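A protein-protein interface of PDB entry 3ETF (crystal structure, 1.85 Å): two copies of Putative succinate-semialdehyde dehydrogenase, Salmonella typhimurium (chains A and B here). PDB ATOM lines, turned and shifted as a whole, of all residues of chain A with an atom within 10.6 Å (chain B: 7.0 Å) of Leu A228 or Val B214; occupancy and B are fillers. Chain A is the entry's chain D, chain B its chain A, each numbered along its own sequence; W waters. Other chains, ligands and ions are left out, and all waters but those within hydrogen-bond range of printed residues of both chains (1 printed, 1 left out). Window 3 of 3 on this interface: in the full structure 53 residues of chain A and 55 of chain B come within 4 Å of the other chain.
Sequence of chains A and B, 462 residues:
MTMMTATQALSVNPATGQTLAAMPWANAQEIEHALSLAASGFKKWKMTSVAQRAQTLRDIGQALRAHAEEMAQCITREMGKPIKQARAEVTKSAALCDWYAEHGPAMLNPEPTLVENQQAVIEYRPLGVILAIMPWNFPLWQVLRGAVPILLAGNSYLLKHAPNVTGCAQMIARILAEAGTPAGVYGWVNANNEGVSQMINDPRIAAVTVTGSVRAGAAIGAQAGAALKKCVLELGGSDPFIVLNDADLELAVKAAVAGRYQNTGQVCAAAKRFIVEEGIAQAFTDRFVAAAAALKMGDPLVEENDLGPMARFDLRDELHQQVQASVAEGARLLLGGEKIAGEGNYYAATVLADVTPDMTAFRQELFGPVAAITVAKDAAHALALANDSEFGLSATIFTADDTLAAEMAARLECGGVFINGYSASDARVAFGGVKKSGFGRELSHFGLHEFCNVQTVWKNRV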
ATOM      1  N   LEU A 127      14.815   2.554  15.680  1.00  0.00           N
ATOM      2  CA  LEU A 127      14.799   3.864  16.296  1.00  0.00           C
ATOM      3  C   LEU A 127      13.446   4.599  16.067  1.00  0.00           C
ATOM      4  O   LEU A 127      12.883   5.221  16.988  1.00  0.00           O
ATOM      5  CB  LEU A 127      15.945   4.660  15.698  1.00  0.00           C
ATOM      6  CG  LEU A 127      16.674   5.806  16.373  1.00  0.00           C
ATOM      7  CD1 LEU A 127      17.184   5.424  17.792  1.00  0.00           C
ATOM      8  CD2 LEU A 127      17.849   6.228  15.493  1.00  0.00           C
ATOM      9  N   MET A 199       9.575  19.350  10.369  1.00  0.00           N
ATOM     10  CA  MET A 199       9.664  17.907  10.562  1.00  0.00           C
ATOM     11  C   MET A 199      10.812  17.529  11.503  1.00  0.00           C
ATOM     12  O   MET A 199      10.632  16.692  12.382  1.00  0.00           O
ATOM     13  CB  MET A 199       9.768  17.187   9.211  1.00  0.00           C
ATOM     14  CG  MET A 199       8.506  17.358   8.377  1.00  0.00           C
ATOM     15  SD  MET A 199       8.590  16.263   6.755  1.00  0.00           S
ATOM     16  CE  MET A 199       9.955  17.269   5.784  1.00  0.00           C
ATOM     17  N   ILE A 200      11.981  18.143  11.323  1.00  0.00           N
ATOM     18  CA  ILE A 200      13.113  17.898  12.232  1.00  0.00           C
ATOM     19  C   ILE A 200      12.718  18.140  13.691  1.00  0.00           C
ATOM     20  O   ILE A 200      13.145  17.407  14.606  1.00  0.00           O
ATOM     21  CB  ILE A 200      14.321  18.780  11.876  1.00  0.00           C
ATOM     22  CG1 ILE A 200      14.856  18.399  10.478  1.00  0.00           C
ATOM     23  CG2 ILE A 200      15.434  18.666  12.973  1.00  0.00           C
ATOM     24  CD1 ILE A 200      15.872  19.409   9.921  1.00  0.00           C
ATOM     25  N   ASN A 201      11.877  19.153  13.897  1.00  0.00           N
ATOM     26  CA  ASN A 201      11.442  19.535  15.238  1.00  0.00           C
ATOM     27  C   ASN A 201      10.230  18.780  15.767  1.00  0.00           C
ATOM     28  O   ASN A 201       9.825  18.980  16.914  1.00  0.00           O
ATOM     29  CB  ASN A 201      11.265  21.056  15.316  1.00  0.00           C
ATOM     30  CG  ASN A 201      12.598  21.780  15.268  1.00  0.00           C
ATOM     31  OD1 ASN A 201      12.870  22.562  14.359  1.00  0.00           O
ATOM     32  ND2 ASN A 201      13.458  21.479  16.217  1.00  0.00           N
ATOM     33  N   ASP A 202       9.665  17.908  14.935  1.00  0.00           N
ATOM     34  CA  ASP A 202       8.524  17.082  15.322  1.00  0.00           C
ATOM     35  C   ASP A 202       9.001  15.803  16.021  1.00  0.00           C
ATOM     36  O   ASP A 202       9.912  15.143  15.531  1.00  0.00           O
ATOM     37  CB  ASP A 202       7.676  16.730  14.087  1.00  0.00           C
ATOM     38  CG  ASP A 202       6.318  16.132  14.457  1.00  0.00           C
ATOM     39  OD1 ASP A 202       6.274  14.957  14.881  1.00  0.00           O
ATOM     40  OD2 ASP A 202       5.282  16.837  14.281  1.00  0.00           O
ATOM     41  N   PRO A 203       8.377  15.442  17.167  1.00  0.00           N
ATOM     42  CA  PRO A 203       8.782  14.236  17.917  1.00  0.00           C
ATOM     43  C   PRO A 203       8.647  12.923  17.154  1.00  0.00           C
ATOM     44  O   PRO A 203       9.276  11.931  17.537  1.00  0.00           O
ATOM     45  CB  PRO A 203       7.852  14.241  19.134  1.00  0.00           C
ATOM     46  CG  PRO A 203       6.701  15.137  18.735  1.00  0.00           C
ATOM     47  CD  PRO A 203       7.292  16.171  17.852  1.00  0.00           C
ATOM     48  N   ILE A 205       9.808  12.440  14.162  1.00  0.00           N
ATOM     49  CA  ILE A 205      11.106  12.199  13.504  1.00  0.00           C
ATOM     50  C   ILE A 205      12.135  11.829  14.587  1.00  0.00           C
ATOM     51  O   ILE A 205      12.355  12.599  15.518  1.00  0.00           O
ATOM     52  CB  ILE A 205      11.570  13.416  12.669  1.00  0.00           C
ATOM     53  CG1 ILE A 205      10.586  13.645  11.504  1.00  0.00           C
ATOM     54  CG2 ILE A 205      13.031  13.237  12.198  1.00  0.00           C
ATOM     55  CD1 ILE A 205      10.347  12.401  10.612  1.00  0.00           C
ATOM     56  N   ALA A 206      12.719  10.638  14.471  1.00  0.00           N
ATOM     57  CA  ALA A 206      13.699  10.133  15.447  1.00  0.00           C
ATOM     58  C   ALA A 206      15.127  10.585  15.157  1.00  0.00           C
ATOM     59  O   ALA A 206      15.896  10.875  16.078  1.00  0.00           O
ATOM     60  CB  ALA A 206      13.627   8.599  15.506  1.00  0.00           C
ATOM     61  N   ALA A 207      15.491  10.663  13.875  1.00  0.00           N
ATOM     62  CA  ALA A 207      16.857  11.008  13.460  1.00  0.00           C
ATOM     63  C   ALA A 207      16.833  11.504  12.011  1.00  0.00           C
ATOM     64  O   ALA A 207      15.799  11.422  11.344  1.00  0.00           O
ATOM     65  CB  ALA A 207      17.784   9.776  13.571  1.00  0.00           C
ATOM     66  N   VAL A 208      17.978  11.979  11.518  1.00  0.00           N
ATOM     67  CA  VAL A 208      18.023  12.601  10.182  1.00  0.00           C
ATOM     68  C   VAL A 208      19.220  12.101   9.403  1.00  0.00           C
ATOM     69  O   VAL A 208      20.276  11.848   9.976  1.00  0.00           O
ATOM     70  CB  VAL A 208      18.169  14.149  10.284  1.00  0.00           C
ATOM     71  CG1 VAL A 208      18.085  14.783   8.892  1.00  0.00           C
ATOM     72  CG2 VAL A 208      17.113  14.754  11.217  1.00  0.00           C
ATOM     73  N   ILE A 220      21.060  21.752   8.363  1.00  0.00           N
ATOM     74  CA  ILE A 220      20.268  20.645   8.874  1.00  0.00           C
ATOM     75  C   ILE A 220      20.905  20.061  10.131  1.00  0.00           C
ATOM     76  O   ILE A 220      20.207  19.776  11.099  1.00  0.00           O
ATOM     77  CB  ILE A 220      20.058  19.557   7.795  1.00  0.00           C
ATOM     78  CG1 ILE A 220      19.169  20.133   6.670  1.00  0.00           C
ATOM     79  CG2 ILE A 220      19.391  18.305   8.405  1.00  0.00           C
ATOM     80  CD1 ILE A 220      19.327  19.430   5.344  1.00  0.00           C
ATOM     81  N   GLY A 221      22.228  19.877  10.102  1.00  0.00           N
ATOM     82  CA  GLY A 221      22.954  19.369  11.277  1.00  0.00           C
ATOM     83  C   GLY A 221      22.690  20.223  12.516  1.00  0.00           C
ATOM     84  O   GLY A 221      22.469  19.687  13.603  1.00  0.00           O
ATOM     85  N   ALA A 222      22.710  21.546  12.351  1.00  0.00           N
ATOM     86  CA  ALA A 222      22.422  22.483  13.449  1.00  0.00           C
ATOM     87  C   ALA A 222      21.014  22.288  14.008  1.00  0.00           C
ATOM     88  O   ALA A 222      20.810  22.326  15.234  1.00  0.00           O
ATOM     89  CB  ALA A 222      22.602  23.944  12.996  1.00  0.00           C
ATOM     90  N   GLN A 223      20.045  22.086  13.121  1.00  0.00           N
ATOM     91  CA  GLN A 223      18.654  21.870  13.568  1.00  0.00           C
ATOM     92  C   GLN A 223      18.498  20.533  14.290  1.00  0.00           C
ATOM     93  O   GLN A 223      17.835  20.451  15.337  1.00  0.00           O
ATOM     94  CB  GLN A 223      17.665  21.976  12.395  1.00  0.00           C
ATOM     95  CG  GLN A 223      17.889  23.219  11.498  1.00  0.00           C
ATOM     96  CD  GLN A 223      16.828  23.378  10.410  1.00  0.00           C
ATOM     97  OE1 GLN A 223      15.638  23.430  10.726  1.00  0.00           O
ATOM     98  NE2 GLN A 223      17.248  23.494   9.126  1.00  0.00           N
ATOM     99  N   ALA A 224      19.098  19.484  13.738  1.00  0.00           N
ATOM    100  CA  ALA A 224      19.011  18.150  14.352  1.00  0.00           C
ATOM    101  C   ALA A 224      19.663  18.148  15.739  1.00  0.00           C
ATOM    102  O   ALA A 224      19.100  17.614  16.694  1.00  0.00           O
ATOM    103  CB  ALA A 224      19.659  17.102  13.463  1.00  0.00           C
ATOM    104  N   GLY A 225      20.844  18.762  15.830  1.00  0.00           N
ATOM    105  CA  GLY A 225      21.575  18.871  17.086  1.00  0.00           C
ATOM    106  C   GLY A 225      20.725  19.572  18.134  1.00  0.00           C
ATOM    107  O   GLY A 225      20.602  19.088  19.257  1.00  0.00           O
ATOM    108  N   ALA A 226      20.116  20.696  17.759  1.00  0.00           N
ATOM    109  CA  ALA A 226      19.265  21.455  18.703  1.00  0.00           C
ATOM    110  C   ALA A 226      18.065  20.656  19.171  1.00  0.00           C
ATOM    111  O   ALA A 226      17.581  20.858  20.288  1.00  0.00           O
ATOM    112  CB  ALA A 226      18.809  22.791  18.076  1.00  0.00           C
ATOM    113  N   ALA A 227      17.589  19.746  18.322  1.00  0.00           N
ATOM    114  CA  ALA A 227      16.457  18.866  18.650  1.00  0.00           C
ATOM    115  C   ALA A 227      16.885  17.550  19.314  1.00  0.00           C
ATOM    116  O   ALA A 227      16.058  16.689  19.601  1.00  0.00           O
ATOM    117  CB  ALA A 227      15.635  18.596  17.405  1.00  0.00           C
ATOM    118  N   LEU A 228      18.189  17.406  19.566  1.00  0.00           N
ATOM    119  CA  LEU A 228      18.742  16.207  20.216  1.00  0.00           C
ATOM    120  C   LEU A 228      18.561  14.944  19.377  1.00  0.00           C
ATOM    121  O   LEU A 228      18.358  13.845  19.902  1.00  0.00           O
ATOM    122  CB  LEU A 228      18.174  16.016  21.629  1.00  0.00           C
ATOM    123  CG  LEU A 228      18.411  17.242  22.534  1.00  0.00           C
ATOM    124  CD1 LEU A 228      17.845  16.992  23.897  1.00  0.00           C
ATOM    125  CD2 LEU A 228      19.878  17.616  22.625  1.00  0.00           C
ATOM    126  N   LYS A 229      18.654  15.104  18.062  1.00  0.00           N
ATOM    127  CA  LYS A 229      18.493  13.979  17.160  1.00  0.00           C
ATOM    128  C   LYS A 229      19.766  13.742  16.384  1.00  0.00           C
ATOM    129  O   LYS A 229      20.414  14.683  15.929  1.00  0.00           O
ATOM    130  CB  LYS A 229      17.345  14.252  16.201  1.00  0.00           C
ATOM    131  CG  LYS A 229      16.040  14.383  16.977  1.00  0.00           C
ATOM    132  CD  LYS A 229      14.875  14.726  16.113  1.00  0.00           C
ATOM    133  CE  LYS A 229      13.699  15.035  17.020  1.00  0.00           C
ATOM    134  NZ  LYS A 229      12.487  15.341  16.222  1.00  0.00           N
ATOM    135  N   LYS A 230      20.135  12.481  16.253  1.00  0.00           N
ATOM    136  CA  LYS A 230      21.386  12.184  15.583  1.00  0.00           C
ATOM    137  C   LYS A 230      21.246  12.324  14.089  1.00  0.00           C
ATOM    138  O   LYS A 230      20.145  12.206  13.546  1.00  0.00           O
ATOM    139  CB  LYS A 230      21.934  10.794  15.948  1.00  0.00           C
ATOM    140  CG  LYS A 230      21.301   9.627  15.309  1.00  0.00           C
ATOM    141  CD  LYS A 230      22.211   8.399  15.472  1.00  0.00           C
ATOM    142  CE  LYS A 230      23.436   8.430  14.538  1.00  0.00           C
ATOM    143  NZ  LYS A 230      24.266   7.198  14.705  1.00  0.00           N
ATOM    144  N   CYS A 231      22.373  12.628  13.441  1.00  0.00           N
ATOM    145  CA  CYS A 231      22.462  12.698  11.986  1.00  0.00           C
ATOM    146  C   CYS A 231      23.552  11.788  11.452  1.00  0.00           C
ATOM    147  O   CYS A 231      24.432  11.311  12.192  1.00  0.00           O
ATOM    148  CB  CYS A 231      22.874  14.100  11.510  1.00  0.00           C
ATOM    149  SG  CYS A 231      21.730  15.439  11.802  1.00  0.00           S
ATOM    150  N   GLY B 212      25.597  15.872  30.324  1.00  0.00           N
ATOM    151  CA  GLY B 212      25.051  16.958  31.157  1.00  0.00           C
ATOM    152  C   GLY B 212      23.564  17.098  30.951  1.00  0.00           C
ATOM    153  O   GLY B 212      22.887  16.121  30.680  1.00  0.00           O
ATOM    154  N   SER B 213      23.074  18.323  31.068  1.00  0.00           N
ATOM    155  CA  SER B 213      21.652  18.574  30.985  1.00  0.00           C
ATOM    156  C   SER B 213      21.190  18.627  29.535  1.00  0.00           C
ATOM    157  O   SER B 213      21.995  18.831  28.611  1.00  0.00           O
ATOM    158  CB  SER B 213      21.325  19.897  31.679  1.00  0.00           C
ATOM    159  OG  SER B 213      21.878  20.977  30.949  1.00  0.00           O
ATOM    160  N   VAL B 214      19.882  18.460  29.365  1.00  0.00           N
ATOM    161  CA  VAL B 214      19.226  18.550  28.062  1.00  0.00           C
ATOM    162  C   VAL B 214      19.457  19.901  27.399  1.00  0.00           C
ATOM    163  O   VAL B 214      19.733  19.959  26.197  1.00  0.00           O
ATOM    164  CB  VAL B 214      17.712  18.196  28.173  1.00  0.00           C
ATOM    165  CG1 VAL B 214      16.971  18.563  26.924  1.00  0.00           C
ATOM    166  CG2 VAL B 214      17.535  16.701  28.449  1.00  0.00           C
ATOM    167  N   ARG B 215      19.363  20.984  28.167  1.00  0.00           N
ATOM    168  CA  ARG B 215      19.605  22.322  27.632  1.00  0.00           C
ATOM    169  C   ARG B 215      21.056  22.497  27.152  1.00  0.00           C
ATOM    170  O   ARG B 215      21.285  23.055  26.079  1.00  0.00           O
ATOM    171  CB  ARG B 215      19.237  23.421  28.653  1.00  0.00           C
ATOM    172  N   ALA B 216      22.024  22.026  27.949  1.00  0.00           N
ATOM    173  CA  ALA B 216      23.449  22.059  27.560  1.00  0.00           C
ATOM    174  C   ALA B 216      23.694  21.239  26.276  1.00  0.00           C
ATOM    175  O   ALA B 216      24.360  21.698  25.343  1.00  0.00           O
ATOM    176  CB  ALA B 216      24.342  21.530  28.707  1.00  0.00           C
ATOM    177  N   GLY B 217      23.155  20.022  26.251  1.00  0.00           N
ATOM    178  CA  GLY B 217      23.263  19.137  25.092  1.00  0.00           C
ATOM    179  C   GLY B 217      22.709  19.762  23.826  1.00  0.00           C
ATOM    180  O   GLY B 217      23.332  19.669  22.765  1.00  0.00           O
ATOM    181  N   ALA B 218      21.552  20.424  23.934  1.00  0.00           N
ATOM    182  CA  ALA B 218      20.948  21.051  22.756  1.00  0.00           C
ATOM    183  C   ALA B 218      21.779  22.219  22.233  1.00  0.00           C
ATOM    184  O   ALA B 218      21.908  22.404  21.011  1.00  0.00           O
ATOM    185  CB  ALA B 218      19.497  21.501  23.049  1.00  0.00           C
ATOM    186  N   ALA B 219      22.321  23.016  23.155  1.00  0.00           N
ATOM    187  CA  ALA B 219      23.106  24.208  22.805  1.00  0.00           C
ATOM    188  C   ALA B 219      24.387  23.805  22.091  1.00  0.00           C
ATOM    189  O   ALA B 219      24.703  24.301  21.004  1.00  0.00           O
ATOM    190  CB  ALA B 219      23.420  25.035  24.081  1.00  0.00           C
ATOM    191  N   GLY B 221      25.084  20.638  20.842  1.00  0.00           N
ATOM    192  CA  GLY B 221      24.756  19.821  19.665  1.00  0.00           C
ATOM    193  C   GLY B 221      24.470  20.693  18.458  1.00  0.00           C
ATOM    194  O   GLY B 221      24.892  20.378  17.348  1.00  0.00           O
ATOM    195  N   ALA B 222      23.737  21.780  18.668  1.00  0.00           N
ATOM    196  CA  ALA B 222      23.468  22.739  17.593  1.00  0.00           C
ATOM    197  C   ALA B 222      24.753  23.369  17.031  1.00  0.00           C
ATOM    198  O   ALA B 222      24.899  23.495  15.815  1.00  0.00           O
ATOM    199  CB  ALA B 222      22.479  23.833  18.069  1.00  0.00           C
ATOM    200  N   LEU B 233      25.911  12.713  22.770  1.00  0.00           N
ATOM    201  CA  LEU B 233      25.223  13.486  23.813  1.00  0.00           C
ATOM    202  C   LEU B 233      24.601  12.521  24.829  1.00  0.00           C
ATOM    203  O   LEU B 233      23.721  11.740  24.472  1.00  0.00           O
ATOM    204  CB  LEU B 233      24.135  14.376  23.199  1.00  0.00           C
ATOM    205  CG  LEU B 233      24.551  15.376  22.101  1.00  0.00           C
ATOM    206  CD1 LEU B 233      23.326  16.171  21.623  1.00  0.00           C
ATOM    207  CD2 LEU B 233      25.655  16.333  22.581  1.00  0.00           C
ATOM    208  N   LEU B 235      22.629  12.721  28.000  1.00  0.00           N
ATOM    209  CA  LEU B 235      21.928  13.755  28.721  1.00  0.00           C
ATOM    210  C   LEU B 235      21.064  13.166  29.862  1.00  0.00           C
ATOM    211  O   LEU B 235      21.266  12.018  30.267  1.00  0.00           O
ATOM    212  CB  LEU B 235      21.143  14.620  27.730  1.00  0.00           C
ATOM    213  CG  LEU B 235      21.995  15.091  26.522  1.00  0.00           C
ATOM    214  CD1 LEU B 235      21.131  15.877  25.549  1.00  0.00           C
ATOM    215  CD2 LEU B 235      23.250  15.901  26.949  1.00  0.00           C
ATOM    216  N   GLY B 236      20.121  13.926  30.371  1.00  0.00           N
ATOM    217  CA  GLY B 236      19.335  13.423  31.518  1.00  0.00           C
ATOM    218  C   GLY B 236      18.451  12.212  31.229  1.00  0.00           C
ATOM    219  O   GLY B 236      18.292  11.791  30.090  1.00  0.00           O
ATOM    220  N   GLY B 237      17.866  11.653  32.282  1.00  0.00           N
ATOM    221  CA  GLY B 237      16.919  10.577  32.104  1.00  0.00           C
ATOM    222  C   GLY B 237      15.815  10.766  33.125  1.00  0.00           C
ATOM    223  O   GLY B 237      15.924  11.597  34.021  1.00  0.00           O
ATOM    224  N   GLU B 365      12.817  15.714  34.750  1.00  0.00           N
ATOM    225  CA  GLU B 365      13.853  14.963  35.457  1.00  0.00           C
ATOM    226  C   GLU B 365      14.013  15.530  36.874  1.00  0.00           C
ATOM    227  O   GLU B 365      14.327  16.706  37.052  1.00  0.00           O
ATOM    228  CB  GLU B 365      15.186  15.013  34.696  1.00  0.00           C
ATOM    229  CG  GLU B 365      16.354  14.428  35.509  1.00  0.00           C
ATOM    230  CD  GLU B 365      17.653  14.299  34.723  1.00  0.00           C
ATOM    231  OE1 GLU B 365      18.000  15.262  34.000  1.00  0.00           O
ATOM    232  OE2 GLU B 365      18.337  13.245  34.852  1.00  0.00           O
ATOM    233  N   GLU B 390       9.641  12.096  27.624  1.00  0.00           N
ATOM    234  CA  GLU B 390      10.490  12.605  26.559  1.00  0.00           C
ATOM    235  C   GLU B 390      11.932  12.142  26.715  1.00  0.00           C
ATOM    236  O   GLU B 390      12.769  12.470  25.886  1.00  0.00           O
ATOM    237  CB  GLU B 390      10.395  14.117  26.413  1.00  0.00           C
ATOM    238  CG  GLU B 390      10.800  14.961  27.590  1.00  0.00           C
ATOM    239  CD  GLU B 390      10.558  16.483  27.306  1.00  0.00           C
ATOM    240  OE1 GLU B 390       9.856  16.807  26.313  1.00  0.00           O
ATOM    241  OE2 GLU B 390      11.100  17.339  28.064  1.00  0.00           O
ATOM    242  N   PHE B 391      12.211  11.408  27.796  1.00  0.00           N
ATOM    243  CA  PHE B 391      13.550  10.843  28.038  1.00  0.00           C
ATOM    244  C   PHE B 391      13.564   9.361  27.715  1.00  0.00           C
ATOM    245  O   PHE B 391      12.508   8.739  27.559  1.00  0.00           O
ATOM    246  CB  PHE B 391      13.952  11.014  29.503  1.00  0.00           C
ATOM    247  CG  PHE B 391      13.951  12.442  29.958  1.00  0.00           C
ATOM    248  CD1 PHE B 391      15.058  13.242  29.758  1.00  0.00           C
ATOM    249  CD2 PHE B 391      12.824  12.988  30.573  1.00  0.00           C
ATOM    250  CE1 PHE B 391      15.052  14.581  30.176  1.00  0.00           C
ATOM    251  CE2 PHE B 391      12.802  14.328  30.984  1.00  0.00           C
ATOM    252  CZ  PHE B 391      13.924  15.110  30.793  1.00  0.00           C
ATOM    253  N   VAL B 434      17.896   7.388  24.149  1.00  0.00           N
ATOM    254  CA  VAL B 434      17.130   7.844  22.971  1.00  0.00           C
ATOM    255  C   VAL B 434      16.323   9.074  23.348  1.00  0.00           C
ATOM    256  O   VAL B 434      16.364   9.510  24.507  1.00  0.00           O
ATOM    257  CB  VAL B 434      16.168   6.732  22.432  1.00  0.00           C
ATOM    258  CG1 VAL B 434      16.949   5.516  21.934  1.00  0.00           C
ATOM    259  CG2 VAL B 434      15.116   6.313  23.483  1.00  0.00           C
ATOM    260  N   LYS B 435      15.589   9.642  22.382  1.00  0.00           N
ATOM    261  CA  LYS B 435      14.768  10.820  22.678  1.00  0.00           C
ATOM    262  C   LYS B 435      15.610  11.950  23.274  1.00  0.00           C
ATOM    263  O   LYS B 435      16.734  12.189  22.824  1.00  0.00           O
ATOM    264  CB  LYS B 435      13.565  10.446  23.579  1.00  0.00           C
ATOM    265  CG  LYS B 435      12.581   9.433  22.948  1.00  0.00           C
ATOM    266  CD  LYS B 435      11.441   9.150  23.933  1.00  0.00           C
ATOM    267  CE  LYS B 435      10.688   7.913  23.592  1.00  0.00           C
ATOM    268  NZ  LYS B 435       9.717   7.544  24.709  1.00  0.00           N
ATOM    269  N   LYS B 436      15.100  12.655  24.282  1.00  0.00           N
ATOM    270  CA  LYS B 436      15.866  13.789  24.824  1.00  0.00           C
ATOM    271  C   LYS B 436      17.029  13.397  25.743  1.00  0.00           C
ATOM    272  O   LYS B 436      17.751  14.267  26.220  1.00  0.00           O
ATOM    273  CB  LYS B 436      14.957  14.848  25.473  1.00  0.00           C
ATOM    274  CG  LYS B 436      13.983  15.474  24.484  1.00  0.00           C
ATOM    275  CD  LYS B 436      13.289  16.683  25.085  1.00  0.00           C
ATOM    276  CE  LYS B 436      12.421  17.386  24.039  1.00  0.00           C
ATOM    277  NZ  LYS B 436      11.749  18.574  24.668  1.00  0.00           N
ATOM    278  N   SER B 437      17.211  12.098  25.998  1.00  0.00           N
ATOM    279  CA  SER B 437      18.410  11.656  26.704  1.00  0.00           C
ATOM    280  C   SER B 437      19.648  11.761  25.795  1.00  0.00           C
ATOM    281  O   SER B 437      20.765  11.550  26.252  1.00  0.00           O
ATOM    282  CB  SER B 437      18.249  10.229  27.231  1.00  0.00           C
ATOM    283  OG  SER B 437      17.191  10.196  28.186  1.00  0.00           O
ATOM    284  N   GLY B 438      19.446  12.054  24.506  1.00  0.00           N
ATOM    285  CA  GLY B 438      20.575  12.263  23.577  1.00  0.00           C
ATOM    286  C   GLY B 438      20.691  11.203  22.494  1.00  0.00           C
ATOM    287  O   GLY B 438      19.691  10.700  21.995  1.00  0.00           O
ATOM    288  N   PHE B 439      21.927  10.882  22.114  1.00  0.00           N
ATOM    289  CA  PHE B 439      22.217   9.863  21.111  1.00  0.00           C
ATOM    290  C   PHE B 439      23.688   9.498  21.203  1.00  0.00           C
ATOM    291  O   PHE B 439      24.471  10.198  21.860  1.00  0.00           O
ATOM    292  CB  PHE B 439      21.864  10.325  19.671  1.00  0.00           C
ATOM    293  CG  PHE B 439      22.445  11.662  19.293  1.00  0.00           C
ATOM    294  CD1 PHE B 439      23.792  11.788  18.952  1.00  0.00           C
ATOM    295  CD2 PHE B 439      21.637  12.795  19.260  1.00  0.00           C
ATOM    296  CE1 PHE B 439      24.326  13.021  18.585  1.00  0.00           C
ATOM    297  CE2 PHE B 439      22.167  14.042  18.910  1.00  0.00           C
ATOM    298  CZ  PHE B 439      23.519  14.149  18.567  1.00  0.00           C
HETATM  299  O   HOH W   1      14.901  13.935  20.524  1.00  0.00           O
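Of chain A, only Leu A228 (3.5 Å) comes within 4 Å of Val B214.
Gly B212 touches none of the printed residues of chain A.
No residue of chain A comes within 4 Å of Ser B213.
No residue of chain A comes within 4 Å of Ala B216.
Of chain A, only Gly A225 (3.97 Å), Ala A226 (3.4 Å) and Leu A228 (3.5 Å) come within 4 Å of Ala B218.
Leu B235 touches just one residue of chain A: Leu A228 (3.6 Å).
Of chain A, only Leu A228 comes within 4 Å of Lys B436.
Of the printed residues of chain B, Ala A222 touches Ala B222.
Of the printed residues of chain A, Phe B439 touches Leu A228, Lys A229 and Lys A230.
Val A208 touches none of the printed residues of chain B.
Gln A223 touches none of the printed residues of chain B.
The nearest residue of chain A that does not touch Val B214 is Ala A226 (6.4 Å).
The nearest printed residue of chain B that does not touch Lys A229 is Lys B435 (5.9 Å).
Ala B222 touches its own counterpart, Ala A222.
Of the 16 pairs that touch across the chains among the printed residues, 1 has its exchanged pair printed and touching as well.
O of Ala B218 touches O of Gly A225, at 3.97 Å.
Gly B221 touches Gly A225 (O to CA, 3.7 Å).
N of Ala B222 touches C of Gly A225 (3.8 Å).
CB of Ala B222 touches CB of Ala A226, at 3.8 Å.
Gly B217 touches Leu A228 (C to CD2, 3.7 Å).
Leu A228 touches Ala B218.
Leu A228 touches Leu B235.
O of Lys B435 touches O of Leu A228, at 3.7 Å.
CD1 of Leu A228 touches O of Lys B436 (3.6 Å).
Phe B439 touches Lys A230 (CD2 to N, 3.4 Å).
Water W1 bridges O of Ala A227 (3.1 Å) and O of Lys B435 (3.4 Å).
N of Leu B235 is in hydrogen-bond range of O of Ser B437, 2.8 Å away.
NZ of Lys B436 is in salt-bridge range of OE1 of Glu B390, at 3.1 Å.
The side-chain amino group (NZ) of Lys A229 lies within hydrogen-bond range of the backbone carbonyl oxygen (O) of Ile A200, 2.7 Å away.
The backbone carbonyl oxygen (O) of Asp A202 lies within hydrogen-bond range of the side-chain amino group (NZ) of Lys A229, at 2.7 Å.
O of Ile A205 sits at hydrogen-bond distance from NZ of Lys A229.
The backbone carbonyl oxygen (O) of Lys A230 sits at hydrogen-bond distance from the backbone NH (N) of Val A208, 3.0 Å away.
Printed residues of chain A that touch a printed residue of chain B: Ala A222, Gly A225, Ala A226, Leu A228, Lys A229 and Lys A230.
Of the 23 printed residues of chain B, 10 touch a printed residue of chain A.
Hydrophobic or aromatic side chains of chain B that line the printed part of chain A: Val B214, Ala B218, Ala B222, Leu B233, Leu B235 and Phe B439.
Among the printed residues, 16 pairs touch across the chains.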
